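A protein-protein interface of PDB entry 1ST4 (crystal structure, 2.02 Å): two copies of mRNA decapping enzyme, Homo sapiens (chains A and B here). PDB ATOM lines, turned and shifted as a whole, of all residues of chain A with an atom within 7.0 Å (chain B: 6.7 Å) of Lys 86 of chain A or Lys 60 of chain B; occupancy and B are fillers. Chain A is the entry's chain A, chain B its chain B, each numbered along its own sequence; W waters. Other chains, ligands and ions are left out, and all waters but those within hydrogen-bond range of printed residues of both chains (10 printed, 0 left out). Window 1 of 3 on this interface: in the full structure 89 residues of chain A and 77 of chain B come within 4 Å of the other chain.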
ATOM      1  N   ARG A  58     -15.788  19.639  30.161  1.00  0.00           N
ATOM      2  CA  ARG A  58     -14.638  19.708  29.293  1.00  0.00           C
ATOM      3  C   ARG A  58     -13.992  18.361  29.081  1.00  0.00           C
ATOM      4  O   ARG A  58     -13.565  18.057  27.971  1.00  0.00           O
ATOM      5  CB  ARG A  58     -13.622  20.659  29.995  1.00  0.00           C
ATOM      6  CG  ARG A  58     -12.257  20.901  29.323  1.00  0.00           C
ATOM      7  CD  ARG A  58     -10.990  20.707  30.264  1.00  0.00           C
ATOM      8  NE  ARG A  58      -9.761  20.433  29.466  1.00  0.00           N
ATOM      9  CZ  ARG A  58      -8.487  20.686  29.825  1.00  0.00           C
ATOM     10  NH1 ARG A  58      -8.197  21.212  31.024  1.00  0.00           N
ATOM     11  NH2 ARG A  58      -7.506  20.410  28.964  1.00  0.00           N
ATOM     12  N   ASP A  59     -13.848  17.556  30.141  1.00  0.00           N
ATOM     13  CA  ASP A  59     -13.090  16.290  30.063  1.00  0.00           C
ATOM     14  C   ASP A  59     -14.086  15.192  29.832  1.00  0.00           C
ATOM     15  O   ASP A  59     -13.725  14.070  29.639  1.00  0.00           O
ATOM     16  CB  ASP A  59     -12.287  15.990  31.364  1.00  0.00           C
ATOM     17  CG  ASP A  59     -10.904  16.591  31.326  1.00  0.00           C
ATOM     18  OD1 ASP A  59     -10.296  16.696  30.225  1.00  0.00           O
ATOM     19  OD2 ASP A  59     -10.369  17.092  32.326  1.00  0.00           O
ATOM     20  N   LYS A  60     -15.364  15.532  29.843  1.00  0.00           N
ATOM     21  CA  LYS A  60     -16.445  14.469  29.615  1.00  0.00           C
ATOM     22  C   LYS A  60     -16.268  13.301  30.628  1.00  0.00           C
ATOM     23  O   LYS A  60     -16.228  12.107  30.295  1.00  0.00           O
ATOM     24  CB  LYS A  60     -16.635  13.995  28.159  1.00  0.00           C
ATOM     25  CG  LYS A  60     -17.024  15.145  27.144  1.00  0.00           C
ATOM     26  CD  LYS A  60     -15.677  15.967  26.813  1.00  0.00           C
ATOM     27  CE  LYS A  60     -15.995  17.028  25.767  1.00  0.00           C
ATOM     28  NZ  LYS A  60     -14.890  18.093  25.581  1.00  0.00           N
ATOM     29  N   ILE A  61     -16.240  13.701  31.896  1.00  0.00           N
ATOM     30  CA  ILE A  61     -16.063  12.705  32.894  1.00  0.00           C
ATOM     31  C   ILE A  61     -16.895  13.056  34.099  1.00  0.00           C
ATOM     32  O   ILE A  61     -17.072  14.223  34.435  1.00  0.00           O
ATOM     33  CB  ILE A  61     -14.586  12.618  33.275  1.00  0.00           C
ATOM     34  CG1 ILE A  61     -14.291  11.457  34.290  1.00  0.00           C
ATOM     35  CG2 ILE A  61     -14.076  13.858  34.071  1.00  0.00           C
ATOM     36  CD1 ILE A  61     -12.581  11.295  34.578  1.00  0.00           C
ATOM     37  N   ILE A  62     -17.277  11.999  34.796  1.00  0.00           N
ATOM     38  CA  ILE A  62     -18.059  12.103  36.008  1.00  0.00           C
ATOM     39  C   ILE A  62     -17.671  11.027  37.090  1.00  0.00           C
ATOM     40  O   ILE A  62     -17.564   9.864  36.796  1.00  0.00           O
ATOM     41  CB  ILE A  62     -19.547  12.039  35.669  1.00  0.00           C
ATOM     42  CG1 ILE A  62     -20.311  12.330  36.958  1.00  0.00           C
ATOM     43  CG2 ILE A  62     -20.009  10.679  35.179  1.00  0.00           C
ATOM     44  CD1 ILE A  62     -21.788  12.543  36.703  1.00  0.00           C
ATOM     45  N   LEU A  84     -17.089   7.432  35.114  1.00  0.00           N
ATOM     46  CA  LEU A  84     -17.427   7.278  33.706  1.00  0.00           C
ATOM     47  C   LEU A  84     -16.784   8.376  32.909  1.00  0.00           C
ATOM     48  O   LEU A  84     -16.841   9.545  33.227  1.00  0.00           O
ATOM     49  CB  LEU A  84     -18.954   7.225  33.441  1.00  0.00           C
ATOM     50  CG  LEU A  84     -19.973   6.249  34.101  1.00  0.00           C
ATOM     51  CD1 LEU A  84     -21.418   6.544  33.545  1.00  0.00           C
ATOM     52  CD2 LEU A  84     -19.829   4.861  33.773  1.00  0.00           C
ATOM     53  N   GLU A  85     -16.087   7.931  31.879  1.00  0.00           N
ATOM     54  CA  GLU A  85     -15.360   8.812  31.021  1.00  0.00           C
ATOM     55  C   GLU A  85     -15.668   8.505  29.590  1.00  0.00           C
ATOM     56  O   GLU A  85     -15.576   7.309  29.109  1.00  0.00           O
ATOM     57  CB  GLU A  85     -13.852   8.808  31.329  1.00  0.00           C
ATOM     58  CG  GLU A  85     -13.109  10.068  30.794  1.00  0.00           C
ATOM     59  CD  GLU A  85     -11.535  10.013  30.977  1.00  0.00           C
ATOM     60  OE1 GLU A  85     -10.840  10.965  30.565  1.00  0.00           O
ATOM     61  OE2 GLU A  85     -11.027   9.051  31.575  1.00  0.00           O
ATOM     62  N   LYS A  86     -16.114   9.561  28.852  1.00  0.00           N
ATOM     63  CA  LYS A  86     -16.261   9.314  27.407  1.00  0.00           C
ATOM     64  C   LYS A  86     -14.840   9.024  26.763  1.00  0.00           C
ATOM     65  O   LYS A  86     -13.836   9.487  27.265  1.00  0.00           O
ATOM     66  CB  LYS A  86     -16.863  10.591  26.739  1.00  0.00           C
ATOM     67  CG  LYS A  86     -18.405  10.900  27.125  1.00  0.00           C
ATOM     68  CD  LYS A  86     -19.370   9.751  26.625  1.00  0.00           C
ATOM     69  CE  LYS A  86     -20.800   9.993  27.108  1.00  0.00           C
ATOM     70  NZ  LYS A  86     -21.262  11.212  26.353  1.00  0.00           N
ATOM     71  N   THR A  87     -14.763   8.243  25.683  1.00  0.00           N
ATOM     72  CA  THR A  87     -13.517   7.852  25.109  1.00  0.00           C
ATOM     73  C   THR A  87     -13.112   8.708  23.855  1.00  0.00           C
ATOM     74  O   THR A  87     -13.964   9.454  23.228  1.00  0.00           O
ATOM     75  CB  THR A  87     -13.542   6.388  24.684  1.00  0.00           C
ATOM     76  OG1 THR A  87     -14.679   6.241  23.823  1.00  0.00           O
ATOM     77  CG2 THR A  87     -13.748   5.391  25.903  1.00  0.00           C
ATOM     78  N   PRO A  88     -11.804   8.713  23.581  1.00  0.00           N
ATOM     79  CA  PRO A  88     -11.237   9.425  22.382  1.00  0.00           C
ATOM     80  C   PRO A  88     -11.807   8.772  21.155  1.00  0.00           C
ATOM     81  O   PRO A  88     -12.247   7.608  21.257  1.00  0.00           O
ATOM     82  CB  PRO A  88      -9.729   9.160  22.453  1.00  0.00           C
ATOM     83  CG  PRO A  88      -9.424   8.694  23.873  1.00  0.00           C
ATOM     84  CD  PRO A  88     -10.749   8.100  24.455  1.00  0.00           C
ATOM     85  N   PHE A  89     -11.936   9.529  20.059  1.00  0.00           N
ATOM     86  CA  PHE A  89     -12.286   8.944  18.790  1.00  0.00           C
ATOM     87  C   PHE A  89     -11.157   8.145  18.197  1.00  0.00           C
ATOM     88  O   PHE A  89      -9.996   8.488  18.463  1.00  0.00           O
ATOM     89  CB  PHE A  89     -12.558  10.097  17.829  1.00  0.00           C
ATOM     90  CG  PHE A  89     -13.865  10.872  18.217  1.00  0.00           C
ATOM     91  CD1 PHE A  89     -13.796  12.019  18.978  1.00  0.00           C
ATOM     92  CD2 PHE A  89     -15.089  10.366  17.923  1.00  0.00           C
ATOM     93  CE1 PHE A  89     -15.018  12.813  19.420  1.00  0.00           C
ATOM     94  CE2 PHE A  89     -16.296  11.157  18.308  1.00  0.00           C
ATOM     95  CZ  PHE A  89     -16.221  12.290  19.050  1.00  0.00           C
ATOM     96  N   ASN A 125     -19.425   4.036  20.845  1.00  0.00           N
ATOM     97  CA  ASN A 125     -20.021   4.577  22.066  1.00  0.00           C
ATOM     98  C   ASN A 125     -19.377   4.172  23.414  1.00  0.00           C
ATOM     99  O   ASN A 125     -19.858   4.534  24.485  1.00  0.00           O
ATOM    100  CB  ASN A 125     -21.513   4.249  22.027  1.00  0.00           C
ATOM    101  CG  ASN A 125     -22.168   4.724  20.675  1.00  0.00           C
ATOM    102  OD1 ASN A 125     -21.685   5.696  20.061  1.00  0.00           O
ATOM    103  ND2 ASN A 125     -23.299   4.079  20.271  1.00  0.00           N
ATOM    104  N   ASP A 126     -18.254   3.444  23.334  1.00  0.00           N
ATOM    105  CA  ASP A 126     -17.546   2.913  24.524  1.00  0.00           C
ATOM    106  C   ASP A 126     -17.342   3.989  25.520  1.00  0.00           C
ATOM    107  O   ASP A 126     -16.830   5.043  25.140  1.00  0.00           O
ATOM    108  CB  ASP A 126     -16.144   2.441  24.018  1.00  0.00           C
ATOM    109  CG  ASP A 126     -15.368   1.609  25.098  1.00  0.00           C
ATOM    110  OD1 ASP A 126     -15.717   1.596  26.340  1.00  0.00           O
ATOM    111  OD2 ASP A 126     -14.399   0.867  24.755  1.00  0.00           O
ATOM    112  N   VAL A 127     -17.764   3.743  26.764  1.00  0.00           N
ATOM    113  CA  VAL A 127     -17.481   4.577  27.910  1.00  0.00           C
ATOM    114  C   VAL A 127     -16.615   3.817  28.894  1.00  0.00           C
ATOM    115  O   VAL A 127     -16.882   2.652  29.275  1.00  0.00           O
ATOM    116  CB  VAL A 127     -18.790   4.879  28.613  1.00  0.00           C
ATOM    117  CG1 VAL A 127     -18.587   5.526  30.061  1.00  0.00           C
ATOM    118  CG2 VAL A 127     -19.592   5.870  27.676  1.00  0.00           C
ATOM    119  N   LYS A 128     -15.576   4.480  29.272  1.00  0.00           N
ATOM    120  CA  LYS A 128     -14.578   3.916  30.112  1.00  0.00           C
ATOM    121  C   LYS A 128     -15.126   4.049  31.553  1.00  0.00           C
ATOM    122  O   LYS A 128     -15.359   5.210  32.059  1.00  0.00           O
ATOM    123  CB  LYS A 128     -13.251   4.727  29.893  1.00  0.00           C
ATOM    124  CG  LYS A 128     -12.203   4.336  30.880  1.00  0.00           C
ATOM    125  CD  LYS A 128     -11.211   5.517  31.235  1.00  0.00           C
ATOM    126  CE  LYS A 128     -10.449   5.817  29.942  1.00  0.00           C
ATOM    127  NZ  LYS A 128      -9.543   6.992  29.857  1.00  0.00           N
ATOM    128  N   PHE A 285      -0.729  13.243  24.015  1.00  0.00           N
ATOM    129  CA  PHE A 285      -1.843  13.171  24.999  1.00  0.00           C
ATOM    130  C   PHE A 285      -1.599  14.145  26.145  1.00  0.00           C
ATOM    131  O   PHE A 285      -0.660  13.949  26.908  1.00  0.00           O
ATOM    132  CB  PHE A 285      -1.952  11.757  25.572  1.00  0.00           C
ATOM    133  CG  PHE A 285      -3.037  11.544  26.653  1.00  0.00           C
ATOM    134  CD1 PHE A 285      -2.824  10.578  27.637  1.00  0.00           C
ATOM    135  CD2 PHE A 285      -4.289  12.132  26.593  1.00  0.00           C
ATOM    136  CE1 PHE A 285      -3.811  10.249  28.624  1.00  0.00           C
ATOM    137  CE2 PHE A 285      -5.227  11.895  27.611  1.00  0.00           C
ATOM    138  CZ  PHE A 285      -5.034  10.929  28.568  1.00  0.00           C
ATOM    139  N   SER B  56      -7.514  15.915  20.072  1.00  0.00           N
ATOM    140  CA  SER B  56      -7.176  15.920  21.463  1.00  0.00           C
ATOM    141  C   SER B  56      -7.831  14.736  22.114  1.00  0.00           C
ATOM    142  O   SER B  56      -9.059  14.745  22.288  1.00  0.00           O
ATOM    143  CB  SER B  56      -7.656  17.186  22.145  1.00  0.00           C
ATOM    144  OG  SER B  56      -7.293  17.096  23.511  1.00  0.00           O
ATOM    145  N   ALA B  57      -7.065  13.715  22.482  1.00  0.00           N
ATOM    146  CA  ALA B  57      -7.669  12.600  23.220  1.00  0.00           C
ATOM    147  C   ALA B  57      -8.162  12.975  24.612  1.00  0.00           C
ATOM    148  O   ALA B  57      -9.130  12.425  25.124  1.00  0.00           O
ATOM    149  CB  ALA B  57      -6.656  11.402  23.303  1.00  0.00           C
ATOM    150  N   ARG B  58      -7.507  13.919  25.234  1.00  0.00           N
ATOM    151  CA  ARG B  58      -7.867  14.397  26.525  1.00  0.00           C
ATOM    152  C   ARG B  58      -9.277  15.045  26.456  1.00  0.00           C
ATOM    153  O   ARG B  58     -10.071  14.824  27.339  1.00  0.00           O
ATOM    154  CB  ARG B  58      -6.866  15.562  26.909  1.00  0.00           C
ATOM    155  CG  ARG B  58      -7.043  16.234  28.287  1.00  0.00           C
ATOM    156  CD  ARG B  58      -7.365  15.209  29.305  1.00  0.00           C
ATOM    157  NE  ARG B  58      -7.841  15.773  30.566  1.00  0.00           N
ATOM    158  CZ  ARG B  58      -7.229  16.664  31.370  1.00  0.00           C
ATOM    159  NH1 ARG B  58      -5.985  17.174  31.151  1.00  0.00           N
ATOM    160  NH2 ARG B  58      -7.882  17.004  32.485  1.00  0.00           N
ATOM    161  N   ASP B  59      -9.535  15.911  25.446  1.00  0.00           N
ATOM    162  CA  ASP B  59     -10.840  16.610  25.316  1.00  0.00           C
ATOM    163  C   ASP B  59     -11.827  15.829  24.453  1.00  0.00           C
ATOM    164  O   ASP B  59     -12.994  16.261  24.305  1.00  0.00           O
ATOM    165  CB  ASP B  59     -10.679  18.027  24.713  1.00  0.00           C
ATOM    166  CG  ASP B  59      -9.708  18.880  25.517  1.00  0.00           C
ATOM    167  OD1 ASP B  59      -9.552  18.664  26.754  1.00  0.00           O
ATOM    168  OD2 ASP B  59      -9.037  19.800  24.999  1.00  0.00           O
ATOM    169  N   LYS B  60     -11.418  14.635  23.958  1.00  0.00           N
ATOM    170  CA  LYS B  60     -12.295  13.769  23.165  1.00  0.00           C
ATOM    171  C   LYS B  60     -12.875  14.571  21.984  1.00  0.00           C
ATOM    172  O   LYS B  60     -14.126  14.669  21.726  1.00  0.00           O
ATOM    173  CB  LYS B  60     -13.376  12.974  24.004  1.00  0.00           C
ATOM    174  CG  LYS B  60     -13.221  12.916  25.581  1.00  0.00           C
ATOM    175  CD  LYS B  60     -11.981  12.214  26.126  1.00  0.00           C
ATOM    176  CE  LYS B  60     -12.055  11.810  27.627  1.00  0.00           C
ATOM    177  NZ  LYS B  60     -11.516  12.731  28.738  1.00  0.00           N
ATOM    178  N   ILE B  61     -11.971  15.166  21.236  1.00  0.00           N
ATOM    179  CA  ILE B  61     -12.384  15.916  20.052  1.00  0.00           C
ATOM    180  C   ILE B  61     -11.433  15.573  18.876  1.00  0.00           C
ATOM    181  O   ILE B  61     -10.200  15.232  19.095  1.00  0.00           O
ATOM    182  CB  ILE B  61     -12.490  17.469  20.390  1.00  0.00           C
ATOM    183  CG1 ILE B  61     -13.180  18.272  19.189  1.00  0.00           C
ATOM    184  CG2 ILE B  61     -11.102  18.069  20.839  1.00  0.00           C
ATOM    185  CD1 ILE B  61     -13.450  19.582  19.575  1.00  0.00           C
ATOM    186  N   ILE B  62     -11.977  15.523  17.643  1.00  0.00           N
ATOM    187  CA  ILE B  62     -11.150  15.491  16.443  1.00  0.00           C
ATOM    188  C   ILE B  62     -11.714  16.470  15.359  1.00  0.00           C
ATOM    189  O   ILE B  62     -12.935  16.484  15.159  1.00  0.00           O
ATOM    190  CB  ILE B  62     -11.243  14.093  15.731  1.00  0.00           C
ATOM    191  CG1 ILE B  62     -12.451  13.399  16.128  1.00  0.00           C
ATOM    192  CG2 ILE B  62      -9.917  13.240  15.748  1.00  0.00           C
ATOM    193  CD1 ILE B  62     -12.961  12.735  15.043  1.00  0.00           C
ATOM    194  N   LEU B  84     -15.864  16.511  15.445  1.00  0.00           N
ATOM    195  CA  LEU B  84     -16.645  15.688  16.348  1.00  0.00           C
ATOM    196  C   LEU B  84     -16.139  15.670  17.746  1.00  0.00           C
ATOM    197  O   LEU B  84     -14.938  15.790  18.029  1.00  0.00           O
ATOM    198  CB  LEU B  84     -16.938  14.319  15.884  1.00  0.00           C
ATOM    199  CG  LEU B  84     -16.778  13.640  14.584  1.00  0.00           C
ATOM    200  CD1 LEU B  84     -18.043  13.102  14.109  1.00  0.00           C
ATOM    201  CD2 LEU B  84     -15.841  14.302  13.518  1.00  0.00           C
ATOM    202  N   GLU B  85     -17.102  15.736  18.650  1.00  0.00           N
ATOM    203  CA  GLU B  85     -16.797  15.959  20.042  1.00  0.00           C
ATOM    204  C   GLU B  85     -17.727  15.151  20.906  1.00  0.00           C
ATOM    205  O   GLU B  85     -18.949  15.245  20.737  1.00  0.00           O
ATOM    206  CB  GLU B  85     -16.805  17.404  20.369  1.00  0.00           C
ATOM    207  CG  GLU B  85     -16.293  17.659  21.814  1.00  0.00           C
ATOM    208  CD  GLU B  85     -16.327  19.100  22.238  1.00  0.00           C
ATOM    209  OE1 GLU B  85     -16.794  19.963  21.459  1.00  0.00           O
ATOM    210  OE2 GLU B  85     -15.818  19.414  23.338  1.00  0.00           O
ATOM    211  N   LYS B  86     -17.189  14.328  21.820  1.00  0.00           N
ATOM    212  CA  LYS B  86     -18.027  13.626  22.803  1.00  0.00           C
ATOM    213  C   LYS B  86     -18.754  14.619  23.738  1.00  0.00           C
ATOM    214  O   LYS B  86     -18.292  15.739  23.910  1.00  0.00           O
ATOM    215  CB  LYS B  86     -17.207  12.575  23.678  1.00  0.00           C
ATOM    216  CG  LYS B  86     -16.455  11.464  22.821  1.00  0.00           C
ATOM    217  CD  LYS B  86     -17.444  10.430  22.270  1.00  0.00           C
ATOM    218  CE  LYS B  86     -16.803   9.399  21.302  1.00  0.00           C
ATOM    219  NZ  LYS B  86     -16.075   8.225  22.073  1.00  0.00           N
ATOM    220  N   THR B  87     -19.894  14.211  24.297  1.00  0.00           N
ATOM    221  CA  THR B  87     -20.653  15.059  25.186  1.00  0.00           C
ATOM    222  C   THR B  87     -20.494  14.697  26.642  1.00  0.00           C
ATOM    223  O   THR B  87     -20.247  13.558  26.986  1.00  0.00           O
ATOM    224  CB  THR B  87     -22.169  14.997  24.881  1.00  0.00           C
ATOM    225  OG1 THR B  87     -22.592  13.636  24.787  1.00  0.00           O
ATOM    226  CG2 THR B  87     -22.484  15.634  23.379  1.00  0.00           C
ATOM    227  N   PRO B  88     -20.664  15.697  27.497  1.00  0.00           N
ATOM    228  CA  PRO B  88     -20.645  15.454  28.927  1.00  0.00           C
ATOM    229  C   PRO B  88     -21.807  14.544  29.347  1.00  0.00           C
ATOM    230  O   PRO B  88     -22.731  14.317  28.586  1.00  0.00           O
ATOM    231  CB  PRO B  88     -20.808  16.884  29.577  1.00  0.00           C
ATOM    232  CG  PRO B  88     -20.825  17.959  28.351  1.00  0.00           C
ATOM    233  CD  PRO B  88     -21.048  17.097  27.126  1.00  0.00           C
ATOM    234  N   PHE B  89     -21.726  14.041  30.580  1.00  0.00           N
ATOM    235  CA  PHE B  89     -22.707  13.063  31.029  1.00  0.00           C
ATOM    236  C   PHE B  89     -23.791  13.935  31.668  1.00  0.00           C
ATOM    237  O   PHE B  89     -23.515  14.997  32.154  1.00  0.00           O
ATOM    238  CB  PHE B  89     -22.138  12.070  32.092  1.00  0.00           C
ATOM    239  CG  PHE B  89     -21.232  11.025  31.507  1.00  0.00           C
ATOM    240  CD1 PHE B  89     -19.850  11.261  31.438  1.00  0.00           C
ATOM    241  CD2 PHE B  89     -21.752   9.832  30.965  1.00  0.00           C
ATOM    242  CE1 PHE B  89     -18.992  10.287  30.899  1.00  0.00           C
ATOM    243  CE2 PHE B  89     -20.936   8.864  30.442  1.00  0.00           C
ATOM    244  CZ  PHE B  89     -19.498   9.139  30.338  1.00  0.00           C
ATOM    245  N   PRO B 120     -23.461   2.209  26.311  1.00  0.00           N
ATOM    246  CA  PRO B 120     -24.732   2.646  26.865  1.00  0.00           C
ATOM    247  C   PRO B 120     -25.868   2.788  25.789  1.00  0.00           C
ATOM    248  O   PRO B 120     -25.621   2.739  24.567  1.00  0.00           O
ATOM    249  CB  PRO B 120     -24.408   4.017  27.450  1.00  0.00           C
ATOM    250  CG  PRO B 120     -22.912   4.336  27.051  1.00  0.00           C
ATOM    251  CD  PRO B 120     -22.518   3.296  26.053  1.00  0.00           C
ATOM    252  N   GLN B 123     -29.310   7.563  24.459  1.00  0.00           N
ATOM    253  CA  GLN B 123     -29.336   8.918  24.988  1.00  0.00           C
ATOM    254  C   GLN B 123     -28.014   9.374  25.602  1.00  0.00           C
ATOM    255  O   GLN B 123     -27.844  10.587  25.797  1.00  0.00           O
ATOM    256  CB  GLN B 123     -30.443   9.073  26.063  1.00  0.00           C
ATOM    257  CG  GLN B 123     -31.064   7.722  26.486  1.00  0.00           C
ATOM    258  CD  GLN B 123     -31.381   7.607  27.984  1.00  0.00           C
ATOM    259  OE1 GLN B 123     -31.792   8.600  28.639  1.00  0.00           O
ATOM    260  NE2 GLN B 123     -31.215   6.389  28.532  1.00  0.00           N
ATOM    261  N   LEU B 124     -27.107   8.435  25.982  1.00  0.00           N
ATOM    262  CA  LEU B 124     -25.834   8.875  26.516  1.00  0.00           C
ATOM    263  C   LEU B 124     -24.812   9.118  25.428  1.00  0.00           C
ATOM    264  O   LEU B 124     -23.701   9.580  25.761  1.00  0.00           O
ATOM    265  CB  LEU B 124     -25.292   7.861  27.544  1.00  0.00           C
ATOM    266  CG  LEU B 124     -26.099   7.981  28.864  1.00  0.00           C
ATOM    267  CD1 LEU B 124     -27.109   6.886  28.956  1.00  0.00           C
ATOM    268  CD2 LEU B 124     -25.253   8.038  30.105  1.00  0.00           C
ATOM    269  N   ASN B 125     -25.173   8.806  24.174  1.00  0.00           N
ATOM    270  CA  ASN B 125     -24.185   8.584  23.070  1.00  0.00           C
ATOM    271  C   ASN B 125     -24.016   9.708  22.093  1.00  0.00           C
ATOM    272  O   ASN B 125     -23.219   9.647  21.161  1.00  0.00           O
ATOM    273  CB  ASN B 125     -24.491   7.333  22.244  1.00  0.00           C
ATOM    274  CG  ASN B 125     -24.588   6.074  23.113  1.00  0.00           C
ATOM    275  OD1 ASN B 125     -24.031   6.030  24.215  1.00  0.00           O
ATOM    276  ND2 ASN B 125     -25.240   5.053  22.619  1.00  0.00           N
ATOM    277  N   ASP B 126     -24.778  10.746  22.314  1.00  0.00           N
ATOM    278  CA  ASP B 126     -24.760  11.872  21.426  1.00  0.00           C
ATOM    279  C   ASP B 126     -23.282  12.358  21.178  1.00  0.00           C
ATOM    280  O   ASP B 126     -22.507  12.557  22.175  1.00  0.00           O
ATOM    281  CB  ASP B 126     -25.615  12.974  22.069  1.00  0.00           C
ATOM    282  CG  ASP B 126     -25.754  14.216  21.184  1.00  0.00           C
ATOM    283  OD1 ASP B 126     -25.983  15.332  21.762  1.00  0.00           O
ATOM    284  OD2 ASP B 126     -25.605  14.215  19.927  1.00  0.00           O
HETATM  285  O   HOH W   1     -23.956   1.613  22.275  1.00  0.00           O
HETATM  286  O   HOH W   2     -20.791   8.248  20.923  1.00  0.00           O
HETATM  287  O   HOH W   3     -15.243   6.571  20.147  1.00  0.00           O
HETATM  288  O   HOH W   4     -17.775   7.542  24.351  1.00  0.00           O
HETATM  289  O   HOH W   5     -19.332  14.973  32.249  1.00  0.00           O
HETATM  290  O   HOH W   6     -21.437   6.715  24.957  1.00  0.00           O
HETATM  291  O   HOH W   7     -10.388  12.131  20.346  1.00  0.00           O
HETATM  292  O   HOH W   8     -20.621  11.059  23.599  1.00  0.00           O
HETATM  293  O   HOH W   9     -26.206   5.547  20.020  1.00  0.00           O
HETATM  294  O   HOH W  10     -23.825  11.831  27.832  1.00  0.00           O
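Water W3 lies within hydrogen-bond range of the side-chain amino group of Lys 86 of chain B (2.7 Å) and the backbone carbonyl oxygen of Pro 88 of chain A (3.4 Å).
Water W10 lies within hydrogen-bond range of O of Pro 88 of chain B, NZ of Lys 86 of chain A and O of Leu 124 of chain B.
Water W1 bridges O of Pro 120 of chain B and ND2 of Asn 125 of chain A.
Lys 60 of chain A touches Lys 86 of chain B, and with the chains exchanged Lys 86 of chain A touches Lys 60 of chain B.
Lys 60 of chain A touches Pro 88 of chain B, but with the chains exchanged Pro 88 of chain A does not touch Lys 60 of chain B (4.3 Å).
Pro 88 of chain B touches Lys 60 of chain A (N to CG, 3.7 Å).
Lys 60 of chain A touches Phe 89 of chain B (O to CE1, 3.4 Å).
CD1 of Phe 89 of chain B touches CG2 of Ile 62 of chain A, 3.8 Å away.
Leu 84 of chain A touches Phe 89 of chain B.
O of Asn 125 of chain A touches CD of Pro 120 of chain B, 3.3 Å away.
Val 127 of chain A touches Phe 89 of chain B.
Lys 86 of chain A touches just these residues of chain B: Lys 60, Lys 86, Thr 87, Phe 89 and Leu 124.
Of chain A, only Asp 59 (2.7 Å), Glu 85 (2.6 Å), Lys 86 (2.9 Å), Thr 87 (3.7 Å) and Phe 89 (3.1 Å) come within 4 Å of Lys 60 of chain B.
Of the printed residues of chain A, Pro 120 of chain B touches Asn 125 (3.3 Å) and Val 127 (3.7 Å).
Of the printed residues of chain B, Thr 87 of chain A touches Lys 60 (3.7 Å) and Lys 86 (2.7 Å).
Ser 56 of chain B touches none of the printed residues of chain A.
Lys 128 of chain A touches none of the printed residues of chain B.
The nearest residue of chain B that does not touch Lys 86 of chain A is Pro 88 of chain B (4.1 Å).
The nearest residue of chain A that does not touch Lys 60 of chain B is Lys 60 of chain A (4.1 Å).
The nearest printed residue of chain B that does not touch Phe 89 of chain A is Ile 61 of chain B (4.1 Å).
Of the 18 printed residues of chain B, 14 touch a printed residue of chain A.
Printed residues of chain B that touch a printed residue of chain A: Ala 57, Arg 58, Asp 59, Lys 60, Ile 62, Leu 84, Glu 85, Lys 86, Thr 87, Pro 88, Phe 89, Pro 120, Leu 124 and Asn 125.
Hydrophobic or aromatic side chains of chain B that line the printed part of chain A: Ala 57, Ile 62, Leu 84, Phe 89 and Pro 120.
Among the printed residues, 32 pairs touch across the chains.
Among the printed residues, Asp or Glu carboxylates within 4 Å of a Lys or Arg side-chain nitrogen of the other chain: Arg 58 of chain A with Asp 59 of chain B (3.2 Å), Asp 59 of chain A with Arg 58 of chain B (2.5 Å), Lys 60 of chain A with Glu 85 of chain B (2.8 Å) and Glu 85 of chain A with Lys 60 of chain B (2.6 Å).
N of Ile 62 of chain A sits at hydrogen-bond distance from O of Leu 84 of chain A (2.9 Å).
NZ of Lys 128 of chain A lies within salt-bridge range of OE2 of Glu 85 of chain A, 3.1 Å away.
The backbone carbonyl oxygen (O) of Asp 126 of chain A sits at hydrogen-bond distance from the side-chain hydroxyl (OG1) of Thr 87 of chain A (2.8 Å).
NH2 of Arg 58 of chain B is in salt-bridge range of OD2 of Asp 59 of chain A (2.5 Å).
NE of Arg 58 of chain A lies within salt-bridge range of OD1 of Asp 59 of chain B, at 3.2 Å.
The backbone carbonyl oxygen (O) of Asp 59 of chain B is in hydrogen-bond range of the side-chain amino group (NZ) of Lys 60 of chain A (2.9 Å).
The backbone carbonyl oxygen (O) of Asp 59 of chain A lies within hydrogen-bond range of the side-chain amino group (NZ) of Lys 60 of chain B (2.7 Å).
The side-chain amino group of Lys 60 of chain B is in salt-bridge range of the side-chain carboxylate of Glu 85 of chain A, at 2.6 Å.
NZ of Lys 60 of chain A is in salt-bridge range of OE2 of Glu 85 of chain B, 2.8 Å away.
The backbone carbonyl oxygen (O) of Thr 87 of chain A sits at hydrogen-bond distance from the side-chain amino group (NZ) of Lys 86 of chain B (2.7 Å).
NZ of Lys 86 of chain A sits at hydrogen-bond distance from O of Thr 87 of chain B.
O of Leu 124 of chain B is in hydrogen-bond range of NZ of Lys 86 of chain A.
ND2 of Asn 125 of chain A lies close to ND2 of Asn 125 of chain B (3.2 Å).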
